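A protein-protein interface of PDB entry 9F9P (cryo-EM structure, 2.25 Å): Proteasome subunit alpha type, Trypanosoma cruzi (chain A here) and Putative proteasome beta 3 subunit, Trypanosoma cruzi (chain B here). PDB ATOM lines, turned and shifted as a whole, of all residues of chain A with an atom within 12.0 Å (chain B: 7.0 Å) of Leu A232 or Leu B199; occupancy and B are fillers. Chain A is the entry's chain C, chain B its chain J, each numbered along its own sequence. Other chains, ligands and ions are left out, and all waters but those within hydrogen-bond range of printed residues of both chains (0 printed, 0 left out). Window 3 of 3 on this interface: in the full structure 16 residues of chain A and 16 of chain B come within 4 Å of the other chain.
Printed residues of chain B within 4 Å of Leu A232: Pro B40 (3.7 Å), Val B186 (3.8 Å), Thr B197 (3.6 Å) and Leu B199 (3.9 Å). Leu B199 touches just one residue of chain A: Leu A232 (3.9 Å). Pro B40 touches just these residues of chain A: Leu A232 and Leu A233. No residue of chain A comes within 4 Å of Ala B187. No residue of chain A comes within 4 Å of Ile B200. Of the printed residues of chain B, Tyr A236 touches Glu B38. Printed residues of chain A within 4 Å of Glu B38: Pro A235 and Tyr A236. Of the printed residues of chain B, Pro A235 touches Glu B38. Printed residues of chain B within 4 Å of Leu A233: Pro B40 (3.5 Å) and Val B186 (3.4 Å). The nearest printed residue of chain B that does not touch Leu A232 is Arg B198 (4.01 Å). The nearest residue of chain A that does not touch Leu B199 is Lys A231 (7.2 Å). The nearest printed residue of chain B that does not touch Pro A235 is Pro B40 (4.3 Å).
CG of Pro B40 touches O of Leu A232, 3.7 Å away. O of Leu A232 touches CG2 of Val B186, at 3.8 Å. Leu A232 touches Thr B197. CD1 of Leu A232 touches N of Leu B199 (3.9 Å). CG of Pro B40 touches O of Leu A233 (3.5 Å). Leu A233 touches Val B186. Glu B38 touches Pro A235.
Printed residues of chain B that touch a printed residue of chain A: Glu B38, Pro B40, Val B186, Thr B197 and Leu B199. Hydrophobic or aromatic side chains of chain B within 4 Å of the printed part of chain A: Pro B40 and Val B186. Along chain B the printed residues that touch a printed residue of chain A span positions 38 to 199. Hydrophobic or aromatic side chains of chain A within 4 Å of the printed part of chain B: Leu A232, Leu A233, Pro A235 and Tyr A236. Among the printed residues, 8 pairs touch across the chains.
The side-chain hydroxyl (OH) of Tyr A236 lies within hydrogen-bond range of the side-chain carboxylate (OE2) of Glu B38 (2.9 Å).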
ATOM      1  N   PRO A 227      13.460 -23.697 -23.395  1.00  0.00           N
ATOM      2  CA  PRO A 227      13.180 -22.256 -23.324  1.00  0.00           C
ATOM      3  C   PRO A 227      13.065 -21.750 -21.879  1.00  0.00           C
ATOM      4  O   PRO A 227      13.894 -22.090 -21.036  1.00  0.00           O
ATOM      5  CB  PRO A 227      11.887 -22.194 -24.165  1.00  0.00           C
ATOM      6  CG  PRO A 227      11.140 -23.468 -23.789  1.00  0.00           C
ATOM      7  CD  PRO A 227      12.232 -24.499 -23.565  1.00  0.00           C
ATOM      8  N   ALA A 228      12.044 -20.921 -21.606  1.00  0.00           N
ATOM      9  CA  ALA A 228      11.725 -20.437 -20.267  1.00  0.00           C
ATOM     10  C   ALA A 228      11.744 -21.579 -19.247  1.00  0.00           C
ATOM     11  O   ALA A 228      11.656 -22.754 -19.603  1.00  0.00           O
ATOM     12  CB  ALA A 228      10.368 -19.759 -20.277  1.00  0.00           C
ATOM     13  N   THR A 229      11.843 -21.205 -17.968  1.00  0.00           N
ATOM     14  CA  THR A 229      11.705 -22.131 -16.854  1.00  0.00           C
ATOM     15  C   THR A 229      11.003 -21.401 -15.711  1.00  0.00           C
ATOM     16  O   THR A 229      11.637 -21.040 -14.721  1.00  0.00           O
ATOM     17  CB  THR A 229      13.071 -22.718 -16.460  1.00  0.00           C
ATOM     18  OG1 THR A 229      14.091 -21.909 -17.048  1.00  0.00           O
ATOM     19  CG2 THR A 229      13.256 -24.151 -16.911  1.00  0.00           C
ATOM     20  N   GLN A 230       9.689 -21.182 -15.867  1.00  0.00           N
ATOM     21  CA  GLN A 230       8.934 -20.312 -14.975  1.00  0.00           C
ATOM     22  C   GLN A 230       8.677 -21.032 -13.652  1.00  0.00           C
ATOM     23  O   GLN A 230       7.654 -21.687 -13.506  1.00  0.00           O
ATOM     24  CB  GLN A 230       7.582 -19.918 -15.575  1.00  0.00           C
ATOM     25  CG  GLN A 230       7.624 -19.469 -17.027  1.00  0.00           C
ATOM     26  CD  GLN A 230       6.498 -20.126 -17.792  1.00  0.00           C
ATOM     27  OE1 GLN A 230       6.389 -21.351 -17.844  1.00  0.00           O
ATOM     28  NE2 GLN A 230       5.628 -19.317 -18.372  1.00  0.00           N
ATOM     29  N   LYS A 231       9.597 -20.890 -12.689  1.00  0.00           N
ATOM     30  CA  LYS A 231       9.463 -21.532 -11.393  1.00  0.00           C
ATOM     31  C   LYS A 231       8.590 -20.700 -10.455  1.00  0.00           C
ATOM     32  O   LYS A 231       8.334 -21.104  -9.320  1.00  0.00           O
ATOM     33  CB  LYS A 231      10.837 -21.785 -10.760  1.00  0.00           C
ATOM     34  CG  LYS A 231      11.610 -22.954 -11.357  1.00  0.00           C
ATOM     35  CD  LYS A 231      13.114 -22.753 -11.328  1.00  0.00           C
ATOM     36  CE  LYS A 231      13.829 -23.453 -12.467  1.00  0.00           C
ATOM     37  NZ  LYS A 231      15.216 -22.954 -12.630  1.00  0.00           N
ATOM     38  N   LEU A 232       8.127 -19.542 -10.918  1.00  0.00           N
ATOM     39  CA  LEU A 232       7.208 -18.733 -10.136  1.00  0.00           C
ATOM     40  C   LEU A 232       5.776 -19.175 -10.397  1.00  0.00           C
ATOM     41  O   LEU A 232       4.980 -19.178  -9.462  1.00  0.00           O
ATOM     42  CB  LEU A 232       7.418 -17.248 -10.459  1.00  0.00           C
ATOM     43  CG  LEU A 232       8.787 -16.709 -10.038  1.00  0.00           C
ATOM     44  CD1 LEU A 232       8.852 -15.179 -10.088  1.00  0.00           C
ATOM     45  CD2 LEU A 232       9.149 -17.225  -8.655  1.00  0.00           C
ATOM     46  N   LEU A 233       5.464 -19.521 -11.654  1.00  0.00           N
ATOM     47  CA  LEU A 233       4.140 -20.006 -12.021  1.00  0.00           C
ATOM     48  C   LEU A 233       4.037 -21.532 -11.870  1.00  0.00           C
ATOM     49  O   LEU A 233       2.968 -22.025 -11.535  1.00  0.00           O
ATOM     50  CB  LEU A 233       3.804 -19.507 -13.430  1.00  0.00           C
ATOM     51  CG  LEU A 233       3.856 -17.981 -13.602  1.00  0.00           C
ATOM     52  CD1 LEU A 233       3.521 -17.545 -15.020  1.00  0.00           C
ATOM     53  CD2 LEU A 233       2.905 -17.278 -12.655  1.00  0.00           C
ATOM     54  N   GLU A 234       5.124 -22.293 -12.063  1.00  0.00           N
ATOM     55  CA  GLU A 234       5.114 -23.732 -11.806  1.00  0.00           C
ATOM     56  C   GLU A 234       6.207 -24.121 -10.811  1.00  0.00           C
ATOM     57  O   GLU A 234       7.228 -24.673 -11.199  1.00  0.00           O
ATOM     58  CB  GLU A 234       5.301 -24.555 -13.086  1.00  0.00           C
ATOM     59  CG  GLU A 234       4.048 -24.683 -13.938  1.00  0.00           C
ATOM     60  CD  GLU A 234       3.970 -23.769 -15.153  1.00  0.00           C
ATOM     61  OE1 GLU A 234       4.831 -23.910 -16.061  1.00  0.00           O
ATOM     62  OE2 GLU A 234       3.031 -22.936 -15.201  1.00  0.00           O
ATOM     63  N   PRO A 235       6.004 -23.904  -9.496  1.00  0.00           N
ATOM     64  CA  PRO A 235       7.012 -24.219  -8.481  1.00  0.00           C
ATOM     65  C   PRO A 235       7.557 -25.645  -8.379  1.00  0.00           C
ATOM     66  O   PRO A 235       8.533 -25.865  -7.677  1.00  0.00           O
ATOM     67  CB  PRO A 235       6.268 -23.951  -7.159  1.00  0.00           C
ATOM     68  CG  PRO A 235       5.208 -22.943  -7.513  1.00  0.00           C
ATOM     69  CD  PRO A 235       4.774 -23.341  -8.909  1.00  0.00           C
ATOM     70  N   TYR A 236       6.892 -26.619  -9.011  1.00  0.00           N
ATOM     71  CA  TYR A 236       7.370 -27.999  -9.019  1.00  0.00           C
ATOM     72  C   TYR A 236       7.611 -28.509 -10.441  1.00  0.00           C
ATOM     73  O   TYR A 236       7.903 -29.690 -10.622  1.00  0.00           O
ATOM     74  CB  TYR A 236       6.364 -28.904  -8.307  1.00  0.00           C
ATOM     75  CG  TYR A 236       6.315 -28.740  -6.814  1.00  0.00           C
ATOM     76  CD1 TYR A 236       7.149 -29.478  -5.985  1.00  0.00           C
ATOM     77  CD2 TYR A 236       5.445 -27.830  -6.231  1.00  0.00           C
ATOM     78  CE1 TYR A 236       7.109 -29.333  -4.599  1.00  0.00           C
ATOM     79  CE2 TYR A 236       5.407 -27.661  -4.853  1.00  0.00           C
ATOM     80  CZ  TYR A 236       6.243 -28.413  -4.033  1.00  0.00           C
ATOM     81  OH  TYR A 236       6.183 -28.243  -2.672  1.00  0.00           O
ATOM     82  N   GLY A 237       7.513 -27.617 -11.441  1.00  0.00           N
ATOM     83  CA  GLY A 237       7.843 -27.956 -12.819  1.00  0.00           C
ATOM     84  C   GLY A 237       9.350 -28.120 -13.030  1.00  0.00           C
ATOM     85  O   GLY A 237      10.130 -27.277 -12.606  1.00  0.00           O
ATOM     86  N   VAL A 238       9.745 -29.223 -13.678  1.00  0.00           N
ATOM     87  CA  VAL A 238      11.142 -29.504 -13.984  1.00  0.00           C
ATOM     88  C   VAL A 238      11.239 -29.821 -15.473  1.00  0.00           C
ATOM     89  O   VAL A 238      10.687 -30.828 -15.911  1.00  0.00           O
ATOM     90  CB  VAL A 238      11.699 -30.671 -13.136  1.00  0.00           C
ATOM     91  CG1 VAL A 238      13.197 -30.863 -13.351  1.00  0.00           C
ATOM     92  CG2 VAL A 238      11.398 -30.513 -11.649  1.00  0.00           C
ATOM     93  N   LEU A 239      11.923 -28.951 -16.233  1.00  0.00           N
ATOM     94  CA  LEU A 239      12.319 -29.244 -17.607  1.00  0.00           C
ATOM     95  C   LEU A 239      13.749 -29.775 -17.613  1.00  0.00           C
ATOM     96  O   LEU A 239      14.488 -29.545 -16.658  1.00  0.00           O
ATOM     97  CB  LEU A 239      12.218 -27.980 -18.470  1.00  0.00           C
ATOM     98  CG  LEU A 239      10.812 -27.550 -18.908  1.00  0.00           C
ATOM     99  CD1 LEU A 239      10.892 -26.363 -19.863  1.00  0.00           C
ATOM    100  CD2 LEU A 239      10.042 -28.699 -19.557  1.00  0.00           C
ATOM    101  N   ASN B  26      -1.737 -17.315  -3.633  1.00  0.00           N
ATOM    102  CA  ASN B  26      -1.037 -18.588  -3.621  1.00  0.00           C
ATOM    103  C   ASN B  26      -1.717 -19.677  -2.768  1.00  0.00           C
ATOM    104  O   ASN B  26      -1.194 -20.776  -2.636  1.00  0.00           O
ATOM    105  CB  ASN B  26       0.346 -18.392  -2.998  1.00  0.00           C
ATOM    106  CG  ASN B  26       1.372 -17.759  -3.906  1.00  0.00           C
ATOM    107  OD1 ASN B  26       1.631 -18.215  -5.010  1.00  0.00           O
ATOM    108  ND2 ASN B  26       2.087 -16.796  -3.374  1.00  0.00           N
ATOM    109  N   GLU B  38       1.790 -22.629  -1.990  1.00  0.00           N
ATOM    110  CA  GLU B  38       2.537 -22.407  -3.215  1.00  0.00           C
ATOM    111  C   GLU B  38       1.700 -22.790  -4.444  1.00  0.00           C
ATOM    112  O   GLU B  38       2.199 -23.431  -5.347  1.00  0.00           O
ATOM    113  CB  GLU B  38       3.738 -23.338  -3.288  1.00  0.00           C
ATOM    114  CG  GLU B  38       4.817 -23.166  -2.239  1.00  0.00           C
ATOM    115  CD  GLU B  38       5.871 -24.279  -2.344  1.00  0.00           C
ATOM    116  OE1 GLU B  38       6.998 -23.999  -2.835  1.00  0.00           O
ATOM    117  OE2 GLU B  38       5.564 -25.447  -1.967  1.00  0.00           O
ATOM    118  N   PRO B  40      -0.096 -20.875  -7.245  1.00  0.00           N
ATOM    119  CA  PRO B  40      -0.665 -19.818  -8.083  1.00  0.00           C
ATOM    120  C   PRO B  40      -1.685 -20.330  -9.104  1.00  0.00           C
ATOM    121  O   PRO B  40      -1.671 -21.493  -9.511  1.00  0.00           O
ATOM    122  CB  PRO B  40       0.587 -19.260  -8.758  1.00  0.00           C
ATOM    123  CG  PRO B  40       1.551 -20.405  -8.780  1.00  0.00           C
ATOM    124  CD  PRO B  40       1.344 -21.065  -7.445  1.00  0.00           C
ATOM    125  N   PHE B 164       2.093  -2.102 -12.217  1.00  0.00           N
ATOM    126  CA  PHE B 164       2.415  -3.187 -11.314  1.00  0.00           C
ATOM    127  C   PHE B 164       2.142  -2.819  -9.848  1.00  0.00           C
ATOM    128  O   PHE B 164       1.502  -3.612  -9.146  1.00  0.00           O
ATOM    129  CB  PHE B 164       3.860  -3.627 -11.505  1.00  0.00           C
ATOM    130  CG  PHE B 164       4.313  -4.585 -10.439  1.00  0.00           C
ATOM    131  CD1 PHE B 164       3.848  -5.885 -10.424  1.00  0.00           C
ATOM    132  CD2 PHE B 164       5.140  -4.167  -9.409  1.00  0.00           C
ATOM    133  CE1 PHE B 164       4.229  -6.763  -9.411  1.00  0.00           C
ATOM    134  CE2 PHE B 164       5.524  -5.050  -8.409  1.00  0.00           C
ATOM    135  CZ  PHE B 164       5.060  -6.349  -8.402  1.00  0.00           C
ATOM    136  N   TYR B 183      -1.214 -15.587   1.400  1.00  0.00           N
ATOM    137  CA  TYR B 183       0.148 -16.101   1.394  1.00  0.00           C
ATOM    138  C   TYR B 183       0.920 -15.504   0.224  1.00  0.00           C
ATOM    139  O   TYR B 183       1.675 -16.177  -0.473  1.00  0.00           O
ATOM    140  CB  TYR B 183       0.197 -17.636   1.459  1.00  0.00           C
ATOM    141  CG  TYR B 183      -0.413 -18.238   2.690  1.00  0.00           C
ATOM    142  CD1 TYR B 183       0.315 -18.403   3.858  1.00  0.00           C
ATOM    143  CD2 TYR B 183      -1.747 -18.580   2.729  1.00  0.00           C
ATOM    144  CE1 TYR B 183      -0.265 -18.908   5.014  1.00  0.00           C
ATOM    145  CE2 TYR B 183      -2.357 -19.045   3.896  1.00  0.00           C
ATOM    146  CZ  TYR B 183      -1.616 -19.200   5.048  1.00  0.00           C
ATOM    147  OH  TYR B 183      -2.210 -19.679   6.208  1.00  0.00           O
ATOM    148  N   GLY B 184       0.759 -14.203   0.022  1.00  0.00           N
ATOM    149  CA  GLY B 184       1.464 -13.502  -1.050  1.00  0.00           C
ATOM    150  C   GLY B 184       0.804 -13.639  -2.422  1.00  0.00           C
ATOM    151  O   GLY B 184      -0.334 -14.078  -2.542  1.00  0.00           O
ATOM    152  N   ALA B 185       1.521 -13.267  -3.464  1.00  0.00           N
ATOM    153  CA  ALA B 185       0.919 -13.275  -4.782  1.00  0.00           C
ATOM    154  C   ALA B 185       1.979 -13.442  -5.835  1.00  0.00           C
ATOM    155  O   ALA B 185       3.134 -13.212  -5.565  1.00  0.00           O
ATOM    156  CB  ALA B 185       0.147 -11.999  -5.005  1.00  0.00           C
ATOM    157  N   VAL B 186       1.565 -13.886  -7.012  1.00  0.00           N
ATOM    158  CA  VAL B 186       2.427 -13.889  -8.184  1.00  0.00           C
ATOM    159  C   VAL B 186       1.822 -12.989  -9.263  1.00  0.00           C
ATOM    160  O   VAL B 186       0.611 -12.988  -9.412  1.00  0.00           O
ATOM    161  CB  VAL B 186       2.607 -15.312  -8.701  1.00  0.00           C
ATOM    162  CG1 VAL B 186       3.394 -15.310  -9.977  1.00  0.00           C
ATOM    163  CG2 VAL B 186       3.359 -16.176  -7.738  1.00  0.00           C
ATOM    164  N   ALA B 187       2.659 -12.286 -10.027  1.00  0.00           N
ATOM    165  CA  ALA B 187       2.210 -11.395 -11.091  1.00  0.00           C
ATOM    166  C   ALA B 187       2.985 -11.612 -12.375  1.00  0.00           C
ATOM    167  O   ALA B 187       4.197 -11.783 -12.330  1.00  0.00           O
ATOM    168  CB  ALA B 187       2.405  -9.971 -10.711  1.00  0.00           C
ATOM    169  N   THR B 197       7.871 -11.752 -14.705  1.00  0.00           N
ATOM    170  CA  THR B 197       7.098 -12.406 -13.663  1.00  0.00           C
ATOM    171  C   THR B 197       7.714 -12.056 -12.317  1.00  0.00           C
ATOM    172  O   THR B 197       8.918 -12.108 -12.192  1.00  0.00           O
ATOM    173  CB  THR B 197       7.056 -13.933 -13.880  1.00  0.00           C
ATOM    174  OG1 THR B 197       6.239 -14.334 -14.980  1.00  0.00           O
ATOM    175  CG2 THR B 197       6.396 -14.636 -12.726  1.00  0.00           C
ATOM    176  N   ARG B 198       6.914 -11.722 -11.308  1.00  0.00           N
ATOM    177  CA  ARG B 198       7.435 -11.390  -9.988  1.00  0.00           C
ATOM    178  C   ARG B 198       6.648 -12.059  -8.867  1.00  0.00           C
ATOM    179  O   ARG B 198       5.446 -12.193  -8.952  1.00  0.00           O
ATOM    180  CB  ARG B 198       7.312  -9.908  -9.656  1.00  0.00           C
ATOM    181  CG  ARG B 198       7.920  -8.975 -10.680  1.00  0.00           C
ATOM    182  CD  ARG B 198       8.159  -7.576 -10.133  1.00  0.00           C
ATOM    183  NE  ARG B 198       9.049  -6.884 -11.064  1.00  0.00           N
ATOM    184  CZ  ARG B 198       8.897  -5.643 -11.500  1.00  0.00           C
ATOM    185  NH1 ARG B 198       8.086  -4.806 -10.875  1.00  0.00           N
ATOM    186  NH2 ARG B 198       9.606  -5.236 -12.539  1.00  0.00           N
ATOM    187  N   LEU B 199       7.345 -12.426  -7.794  1.00  0.00           N
ATOM    188  CA  LEU B 199       6.739 -12.955  -6.589  1.00  0.00           C
ATOM    189  C   LEU B 199       6.684 -11.831  -5.563  1.00  0.00           C
ATOM    190  O   LEU B 199       7.678 -11.192  -5.312  1.00  0.00           O
ATOM    191  CB  LEU B 199       7.560 -14.157  -6.119  1.00  0.00           C
ATOM    192  CG  LEU B 199       7.133 -14.810  -4.792  1.00  0.00           C
ATOM    193  CD1 LEU B 199       5.737 -15.447  -4.865  1.00  0.00           C
ATOM    194  CD2 LEU B 199       8.145 -15.871  -4.339  1.00  0.00           C
ATOM    195  N   ILE B 200       5.493 -11.579  -5.032  1.00  0.00           N
ATOM    196  CA  ILE B 200       5.194 -10.507  -4.099  1.00  0.00           C
ATOM    197  C   ILE B 200       5.070 -11.104  -2.701  1.00  0.00           C
ATOM    198  O   ILE B 200       4.323 -12.060  -2.511  1.00  0.00           O
ATOM    199  CB  ILE B 200       3.849  -9.863  -4.487  1.00  0.00           C
ATOM    200  CG1 ILE B 200       3.777  -9.554  -5.976  1.00  0.00           C
ATOM    201  CG2 ILE B 200       3.558  -8.642  -3.649  1.00  0.00           C
ATOM    202  CD1 ILE B 200       2.404  -9.183  -6.464  1.00  0.00           C
ATOM    203  N   ASN B 201       5.723 -10.477  -1.721  1.00  0.00           N
ATOM    204  CA  ASN B 201       5.662 -10.919  -0.334  1.00  0.00           C
ATOM    205  C   ASN B 201       4.388 -10.413   0.354  1.00  0.00           C
ATOM    206  O   ASN B 201       4.043  -9.252   0.225  1.00  0.00           O
ATOM    207  CB  ASN B 201       6.907 -10.466   0.427  1.00  0.00           C
ATOM    208  CG  ASN B 201       7.051 -11.187   1.745  1.00  0.00           C
ATOM    209  OD1 ASN B 201       6.847 -12.402   1.814  1.00  0.00           O
ATOM    210  ND2 ASN B 201       7.357 -10.444   2.798  1.00  0.00           N
